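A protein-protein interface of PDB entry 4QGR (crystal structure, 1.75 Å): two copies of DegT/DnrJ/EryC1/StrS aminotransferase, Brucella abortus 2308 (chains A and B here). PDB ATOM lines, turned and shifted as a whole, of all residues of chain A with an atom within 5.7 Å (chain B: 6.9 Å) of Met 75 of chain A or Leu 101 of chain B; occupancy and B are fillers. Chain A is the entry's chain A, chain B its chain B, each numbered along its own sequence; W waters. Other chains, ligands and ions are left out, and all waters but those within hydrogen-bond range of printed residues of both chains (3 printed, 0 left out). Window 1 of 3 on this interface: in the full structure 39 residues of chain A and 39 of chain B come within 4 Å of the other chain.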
ATOM      1  N   GLN A  71      12.800 -18.367  17.139  1.00  0.00           N
ATOM      2  CA  GLN A  71      12.555 -19.302  18.219  1.00  0.00           C
ATOM      3  C   GLN A  71      13.804 -20.123  18.546  1.00  0.00           C
ATOM      4  O   GLN A  71      14.138 -20.319  19.712  1.00  0.00           O
ATOM      5  CB  GLN A  71      11.424 -20.255  17.845  1.00  0.00           C
ATOM      6  CG  GLN A  71      11.084 -21.334  18.879  1.00  0.00           C
ATOM      7  CD  GLN A  71       9.935 -22.224  18.388  1.00  0.00           C
ATOM      8  OE1 GLN A  71       9.303 -21.919  17.372  1.00  0.00           O
ATOM      9  NE2 GLN A  71       9.748 -23.373  19.012  1.00  0.00           N
ATOM     10  N   MET A  72      14.455 -20.671  17.534  1.00  0.00           N
ATOM     11  CA  MET A  72      15.533 -21.608  17.831  1.00  0.00           C
ATOM     12  C   MET A  72      16.682 -21.039  18.670  1.00  0.00           C
ATOM     13  O   MET A  72      17.184 -21.719  19.590  1.00  0.00           O
ATOM     14  CB  MET A  72      16.014 -22.303  16.563  1.00  0.00           C
ATOM     15  CG  MET A  72      14.952 -23.249  16.004  1.00  0.00           C
ATOM     16  SD  MET A  72      15.615 -24.238  14.640  1.00  0.00           S
ATOM     17  CE  MET A  72      15.397 -23.189  13.206  1.00  0.00           C
ATOM     18  N   PRO A  73      17.122 -19.800  18.386  1.00  0.00           N
ATOM     19  CA  PRO A  73      18.172 -19.253  19.232  1.00  0.00           C
ATOM     20  C   PRO A  73      17.741 -19.103  20.707  1.00  0.00           C
ATOM     21  O   PRO A  73      18.594 -19.259  21.593  1.00  0.00           O
ATOM     22  CB  PRO A  73      18.451 -17.901  18.609  1.00  0.00           C
ATOM     23  CG  PRO A  73      18.142 -18.097  17.162  1.00  0.00           C
ATOM     24  CD  PRO A  73      16.977 -19.042  17.139  1.00  0.00           C
ATOM     25  N   LEU A  74      16.462 -18.776  20.952  1.00  0.00           N
ATOM     26  CA  LEU A  74      15.981 -18.713  22.339  1.00  0.00           C
ATOM     27  C   LEU A  74      16.070 -20.086  22.987  1.00  0.00           C
ATOM     28  O   LEU A  74      16.456 -20.210  24.170  1.00  0.00           O
ATOM     29  CB  LEU A  74      14.526 -18.212  22.388  1.00  0.00           C
ATOM     30  CG  LEU A  74      14.303 -16.779  21.908  1.00  0.00           C
ATOM     31  CD1 LEU A  74      12.809 -16.449  21.842  1.00  0.00           C
ATOM     32  CD2 LEU A  74      14.952 -15.786  22.832  1.00  0.00           C
ATOM     33  N   MET A  75      15.734 -21.136  22.226  1.00  0.00           N
ATOM     34  CA  MET A  75      15.814 -22.487  22.740  1.00  0.00           C
ATOM     35  C   MET A  75      17.245 -22.899  23.081  1.00  0.00           C
ATOM     36  O   MET A  75      17.502 -23.511  24.143  1.00  0.00           O
ATOM     37  CB  MET A  75      15.197 -23.509  21.787  1.00  0.00           C
ATOM     38  CG  MET A  75      13.715 -23.327  21.537  1.00  0.00           C
ATOM     39  SD  MET A  75      13.098 -24.379  20.243  1.00  0.00           S
ATOM     40  CE  MET A  75      13.287 -26.009  20.923  1.00  0.00           C
ATOM     41  N   THR A  76      18.178 -22.568  22.215  1.00  0.00           N
ATOM     42  CA  THR A  76      19.582 -22.944  22.464  1.00  0.00           C
ATOM     43  C   THR A  76      20.125 -22.275  23.711  1.00  0.00           C
ATOM     44  O   THR A  76      20.992 -22.845  24.367  1.00  0.00           O
ATOM     45  CB  THR A  76      20.542 -22.610  21.311  1.00  0.00           C
ATOM     46  OG1 THR A  76      20.632 -21.193  21.149  1.00  0.00           O
ATOM     47  CG2 THR A  76      20.087 -23.233  20.058  1.00  0.00           C
ATOM     48  N   ARG A  77      19.647 -21.063  24.017  1.00  0.00           N
ATOM     49  CA  ARG A  77      20.089 -20.335  25.207  1.00  0.00           C
ATOM     50  C   ARG A  77      19.338 -20.722  26.448  1.00  0.00           C
ATOM     51  O   ARG A  77      19.599 -20.146  27.504  1.00  0.00           O
ATOM     52  CB  ARG A  77      19.953 -18.815  24.994  1.00  0.00           C
ATOM     53  CG  ARG A  77      21.036 -18.277  24.086  1.00  0.00           C
ATOM     54  CD  ARG A  77      22.371 -18.119  24.808  1.00  0.00           C
ATOM     55  NE  ARG A  77      22.408 -16.956  25.717  1.00  0.00           N
ATOM     56  CZ  ARG A  77      23.491 -16.177  25.886  1.00  0.00           C
ATOM     57  NH1 ARG A  77      24.600 -16.418  25.206  1.00  0.00           N
ATOM     58  NH2 ARG A  77      23.480 -15.157  26.737  1.00  0.00           N
ATOM     59  N   GLY A  78      18.420 -21.676  26.371  1.00  0.00           N
ATOM     60  CA  GLY A  78      17.643 -22.077  27.540  1.00  0.00           C
ATOM     61  C   GLY A  78      16.674 -21.010  28.045  1.00  0.00           C
ATOM     62  O   GLY A  78      16.366 -20.964  29.227  1.00  0.00           O
ATOM     63  N   ILE A  79      16.200 -20.145  27.166  1.00  0.00           N
ATOM     64  CA  ILE A  79      15.308 -19.060  27.570  1.00  0.00           C
ATOM     65  C   ILE A  79      13.881 -19.541  27.611  1.00  0.00           C
ATOM     66  O   ILE A  79      13.405 -20.192  26.677  1.00  0.00           O
ATOM     67  CB  ILE A  79      15.456 -17.834  26.631  1.00  0.00           C
ATOM     68  CG1 ILE A  79      16.833 -17.246  26.823  1.00  0.00           C
ATOM     69  CG2 ILE A  79      14.360 -16.795  26.903  1.00  0.00           C
ATOM     70  CD1 ILE A  79      17.225 -16.220  25.798  1.00  0.00           C
ATOM     71  N   LEU A 101       5.879 -18.457  23.202  1.00  0.00           N
ATOM     72  CA  LEU A 101       5.892 -19.858  22.824  1.00  0.00           C
ATOM     73  C   LEU A 101       6.871 -20.658  23.656  1.00  0.00           C
ATOM     74  O   LEU A 101       6.498 -21.728  24.162  1.00  0.00           O
ATOM     75  CB  LEU A 101       6.193 -20.006  21.345  1.00  0.00           C
ATOM     76  CG  LEU A 101       5.977 -21.418  20.821  1.00  0.00           C
ATOM     77  CD1 LEU A 101       4.494 -21.670  20.651  1.00  0.00           C
ATOM     78  CD2 LEU A 101       6.667 -21.594  19.476  1.00  0.00           C
ATOM     79  N   VAL A 102       8.081 -20.126  23.875  1.00  0.00           N
ATOM     80  CA  VAL A 102       9.074 -20.839  24.725  1.00  0.00           C
ATOM     81  C   VAL A 102       8.841 -20.706  26.232  1.00  0.00           C
ATOM     82  O   VAL A 102       9.599 -21.269  27.033  1.00  0.00           O
ATOM     83  CB  VAL A 102      10.536 -20.508  24.382  1.00  0.00           C
ATOM     84  CG1 VAL A 102      10.826 -20.869  22.929  1.00  0.00           C
ATOM     85  CG2 VAL A 102      10.921 -19.052  24.694  1.00  0.00           C
ATOM     86  N   VAL A 224      19.031 -28.322  16.875  1.00  0.00           N
ATOM     87  CA  VAL A 224      17.675 -27.964  17.237  1.00  0.00           C
ATOM     88  C   VAL A 224      16.715 -28.087  16.057  1.00  0.00           C
ATOM     89  O   VAL A 224      15.557 -28.509  16.227  1.00  0.00           O
ATOM     90  CB  VAL A 224      17.626 -26.527  17.850  1.00  0.00           C
ATOM     91  CG1 VAL A 224      16.200 -26.005  18.000  1.00  0.00           C
ATOM     92  CG2 VAL A 224      18.301 -26.532  19.216  1.00  0.00           C
ATOM     93  N   ILE A 239      15.603 -31.106  23.298  1.00  0.00           N
ATOM     94  CA  ILE A 239      14.328 -30.889  22.653  1.00  0.00           C
ATOM     95  C   ILE A 239      14.591 -30.008  21.449  1.00  0.00           C
ATOM     96  O   ILE A 239      15.265 -28.949  21.553  1.00  0.00           O
ATOM     97  CB  ILE A 239      13.325 -30.175  23.582  1.00  0.00           C
ATOM     98  CG1 ILE A 239      13.057 -31.003  24.867  1.00  0.00           C
ATOM     99  CG2 ILE A 239      12.060 -29.844  22.812  1.00  0.00           C
ATOM    100  CD1 ILE A 239      12.703 -32.457  24.654  1.00  0.00           C
ATOM    101  N   GLY A 240      14.033 -30.411  20.312  1.00  0.00           N
ATOM    102  CA  GLY A 240      14.110 -29.575  19.095  1.00  0.00           C
ATOM    103  C   GLY A 240      12.793 -29.461  18.343  1.00  0.00           C
ATOM    104  O   GLY A 240      11.713 -29.696  18.915  1.00  0.00           O
ATOM    105  N   ILE A 241      12.909 -29.102  17.053  1.00  0.00           N
ATOM    106  CA  ILE A 241      11.768 -28.978  16.161  1.00  0.00           C
ATOM    107  C   ILE A 241      12.127 -29.561  14.786  1.00  0.00           C
ATOM    108  O   ILE A 241      13.229 -30.119  14.605  1.00  0.00           O
ATOM    109  CB  ILE A 241      11.312 -27.518  16.062  1.00  0.00           C
ATOM    110  CG1 ILE A 241      12.442 -26.616  15.535  1.00  0.00           C
ATOM    111  CG2 ILE A 241      10.813 -26.984  17.405  1.00  0.00           C
ATOM    112  CD1 ILE A 241      11.946 -25.220  15.209  1.00  0.00           C
ATOM    113  N   THR B  67       5.458 -32.878  12.549  1.00  0.00           N
ATOM    114  CA  THR B  67       5.761 -32.518  13.917  1.00  0.00           C
ATOM    115  C   THR B  67       4.806 -31.415  14.396  1.00  0.00           C
ATOM    116  O   THR B  67       4.127 -31.556  15.450  1.00  0.00           O
ATOM    117  CB  THR B  67       7.243 -32.134  14.047  1.00  0.00           C
ATOM    118  OG1 THR B  67       8.067 -33.216  13.576  1.00  0.00           O
ATOM    119  CG2 THR B  67       7.619 -31.831  15.481  1.00  0.00           C
ATOM    120  N   GLN B  71       1.931 -30.986  17.451  1.00  0.00           N
ATOM    121  CA  GLN B  71       2.072 -29.924  18.415  1.00  0.00           C
ATOM    122  C   GLN B  71       0.824 -29.050  18.498  1.00  0.00           C
ATOM    123  O   GLN B  71       0.356 -28.703  19.585  1.00  0.00           O
ATOM    124  CB  GLN B  71       3.301 -29.049  18.075  1.00  0.00           C
ATOM    125  CG  GLN B  71       3.514 -27.845  18.983  1.00  0.00           C
ATOM    126  CD  GLN B  71       4.644 -26.936  18.480  1.00  0.00           C
ATOM    127  OE1 GLN B  71       5.406 -27.306  17.583  1.00  0.00           O
ATOM    128  NE2 GLN B  71       4.696 -25.731  18.978  1.00  0.00           N
ATOM    129  N   ALA B  96       6.910 -37.757  21.071  1.00  0.00           N
ATOM    130  CA  ALA B  96       7.204 -37.311  22.448  1.00  0.00           C
ATOM    131  C   ALA B  96       7.719 -35.887  22.510  1.00  0.00           C
ATOM    132  O   ALA B  96       7.412 -35.138  23.447  1.00  0.00           O
ATOM    133  CB  ALA B  96       8.258 -38.236  23.090  1.00  0.00           C
ATOM    134  N   GLU B  97       8.527 -35.518  21.527  1.00  0.00           N
ATOM    135  CA  GLU B  97       9.181 -34.199  21.536  1.00  0.00           C
ATOM    136  C   GLU B  97       8.179 -33.057  21.695  1.00  0.00           C
ATOM    137  O   GLU B  97       8.411 -32.094  22.462  1.00  0.00           O
ATOM    138  CB  GLU B  97       9.964 -34.018  20.253  1.00  0.00           C
ATOM    139  CG  GLU B  97      10.770 -32.719  20.147  1.00  0.00           C
ATOM    140  CD  GLU B  97      11.464 -32.658  18.798  1.00  0.00           C
ATOM    141  OE1 GLU B  97      10.753 -32.751  17.749  1.00  0.00           O
ATOM    142  OE2 GLU B  97      12.728 -32.607  18.774  1.00  0.00           O
ATOM    143  N   VAL B  98       7.070 -33.147  20.969  1.00  0.00           N
ATOM    144  CA  VAL B  98       6.120 -32.028  20.960  1.00  0.00           C
ATOM    145  C   VAL B  98       5.475 -31.873  22.321  1.00  0.00           C
ATOM    146  O   VAL B  98       5.032 -30.789  22.647  1.00  0.00           O
ATOM    147  CB  VAL B  98       5.008 -32.168  19.880  1.00  0.00           C
ATOM    148  CG1 VAL B  98       5.582 -32.143  18.481  1.00  0.00           C
ATOM    149  CG2 VAL B  98       4.187 -33.430  20.079  1.00  0.00           C
ATOM    150  N   VAL B  99       5.410 -32.964  23.102  1.00  0.00           N
ATOM    151  CA  VAL B  99       4.843 -32.914  24.440  1.00  0.00           C
ATOM    152  C   VAL B  99       5.767 -32.082  25.320  1.00  0.00           C
ATOM    153  O   VAL B  99       5.309 -31.172  26.027  1.00  0.00           O
ATOM    154  CB  VAL B  99       4.636 -34.331  25.006  1.00  0.00           C
ATOM    155  CG1 VAL B  99       4.279 -34.282  26.476  1.00  0.00           C
ATOM    156  CG2 VAL B  99       3.594 -35.068  24.167  1.00  0.00           C
ATOM    157  N   ALA B 100       7.066 -32.381  25.240  1.00  0.00           N
ATOM    158  CA  ALA B 100       8.093 -31.608  25.943  1.00  0.00           C
ATOM    159  C   ALA B 100       8.100 -30.167  25.512  1.00  0.00           C
ATOM    160  O   ALA B 100       8.269 -29.266  26.334  1.00  0.00           O
ATOM    161  CB  ALA B 100       9.476 -32.190  25.699  1.00  0.00           C
ATOM    162  N   LEU B 101       7.920 -29.939  24.221  1.00  0.00           N
ATOM    163  CA  LEU B 101       8.054 -28.618  23.694  1.00  0.00           C
ATOM    164  C   LEU B 101       6.995 -27.659  24.248  1.00  0.00           C
ATOM    165  O   LEU B 101       7.288 -26.496  24.455  1.00  0.00           O
ATOM    166  CB  LEU B 101       7.984 -28.664  22.185  1.00  0.00           C
ATOM    167  CG  LEU B 101       8.346 -27.343  21.552  1.00  0.00           C
ATOM    168  CD1 LEU B 101       9.845 -27.113  21.455  1.00  0.00           C
ATOM    169  CD2 LEU B 101       7.751 -27.381  20.171  1.00  0.00           C
ATOM    170  N   VAL B 102       5.767 -28.140  24.472  1.00  0.00           N
ATOM    171  CA  VAL B 102       4.713 -27.323  25.080  1.00  0.00           C
ATOM    172  C   VAL B 102       4.770 -27.234  26.604  1.00  0.00           C
ATOM    173  O   VAL B 102       3.924 -26.596  27.212  1.00  0.00           O
ATOM    174  CB  VAL B 102       3.304 -27.821  24.661  1.00  0.00           C
ATOM    175  CG1 VAL B 102       3.147 -27.694  23.161  1.00  0.00           C
ATOM    176  CG2 VAL B 102       3.038 -29.266  25.080  1.00  0.00           C
ATOM    177  N   GLY B 103       5.742 -27.893  27.208  1.00  0.00           N
ATOM    178  CA  GLY B 103       5.916 -27.889  28.649  1.00  0.00           C
ATOM    179  C   GLY B 103       5.319 -29.052  29.431  1.00  0.00           C
ATOM    180  O   GLY B 103       5.506 -29.098  30.651  1.00  0.00           O
ATOM    181  N   ALA B 104       4.612 -29.966  28.770  1.00  0.00           N
ATOM    182  CA  ALA B 104       4.063 -31.147  29.407  1.00  0.00           C
ATOM    183  C   ALA B 104       5.132 -32.245  29.437  1.00  0.00           C
ATOM    184  O   ALA B 104       6.264 -32.043  28.976  1.00  0.00           O
ATOM    185  CB  ALA B 104       2.824 -31.623  28.659  1.00  0.00           C
ATOM    186  N   TYR B 336      11.985 -38.743  31.775  1.00  0.00           N
ATOM    187  CA  TYR B 336      10.518 -38.809  31.876  1.00  0.00           C
ATOM    188  C   TYR B 336      10.039 -40.170  32.385  1.00  0.00           C
ATOM    189  O   TYR B 336      10.756 -41.150  32.288  1.00  0.00           O
ATOM    190  CB  TYR B 336       9.850 -38.476  30.524  1.00  0.00           C
ATOM    191  CG  TYR B 336      10.076 -37.050  30.090  1.00  0.00           C
ATOM    192  CD1 TYR B 336       9.675 -35.983  30.897  1.00  0.00           C
ATOM    193  CD2 TYR B 336      10.694 -36.755  28.875  1.00  0.00           C
ATOM    194  CE1 TYR B 336       9.897 -34.673  30.517  1.00  0.00           C
ATOM    195  CE2 TYR B 336      10.906 -35.457  28.490  1.00  0.00           C
ATOM    196  CZ  TYR B 336      10.514 -34.420  29.315  1.00  0.00           C
ATOM    197  OH  TYR B 336      10.726 -33.135  28.912  1.00  0.00           O
HETATM  198  O   HOH W   1      14.083 -33.837  20.927  1.00  0.00           O
HETATM  199  O   HOH W   2       9.070 -30.555  18.434  1.00  0.00           O
HETATM  200  O   HOH W   3       7.507 -25.075  17.770  1.00  0.00           O
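N of Gly 240 of chain A lies within hydrogen-bond range of OE2 of Glu 97 of chain B, 3.0 Å away.
The side-chain sulfur (SD) of Met 75 of chain A is in hydrogen-bond range of the side-chain amide nitrogen (NE2) of Gln 71 of chain A (3.7 Å).
The backbone carbonyl oxygen (O) of Val 224 of chain A is in hydrogen-bond range of the backbone NH (N) of Ile 241 of chain A (2.8 Å).
CD1 of Leu 101 of chain B touches CE of Met 75 of chain A (3.7 Å).
CD1 of Ile 239 of chain A touches CB of Ala 100 of chain B, 3.4 Å away.
Leu 101 of chain B touches Ile 239 of chain A (CD1 to CG2, 3.8 Å).
Ile 241 of chain A touches Glu 97 of chain B.
Of chain B, only Leu 101 comes within 4 Å of Met 75 of chain A.
Printed residues of chain B within 4 Å of Ile 239 of chain A: Ala 100 (3.4 Å) and Leu 101 (3.8 Å).
Printed residues of chain B within 4 Å of Gly 240 of chain A: Glu 97 (3.0 Å).
Printed residues of chain B within 4 Å of Ile 241 of chain A: Glu 97 (3.9 Å).
Of the printed residues of chain A, Glu 97 of chain B touches Gly 240 (3.0 Å) and Ile 241 (3.9 Å).
Of the printed residues of chain A, Ala 100 of chain B touches Ile 239 (3.4 Å).
Leu 101 of chain B touches just these residues of chain A: Met 75 (3.7 Å) and Ile 239 (3.8 Å).
The nearest printed residue of chain B that does not touch Ile 241 of chain A is Leu 101 of chain B (4.1 Å).
Hydrophobic or aromatic side chains of chain A within 4 Å of the printed part of chain B: Met 75 and Ile 239.
Hydrophobic or aromatic side chains of chain B within 4 Å of the printed part of chain A: Ala 100 and Leu 101.
Among the printed residues, 5 pairs touch across the chains.
Positions printed for both chains: 71, 101 and 102.
Of the 5 pairs that touch across the chains among the printed residues, none has its exchanged pair printed and touching as well.
Water W2 bridges the backbone carbonyl oxygen (O) of Gly 240 of chain A (2.8 Å) and the side-chain carboxylate (OE1) of Glu 97 of chain B (2.9 Å).
Water W1 bridges the side-chain carboxylate of Glu 97 of chain B (2.8 Å) and the backbone NH of Gly 240 of chain A (3.5 Å).
Water W3 lies within hydrogen-bond range of the side-chain amide oxygen of Gln 71 of chain B (3.1 Å) and the side-chain amide nitrogen of Gln 71 of chain A (3.1 Å).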
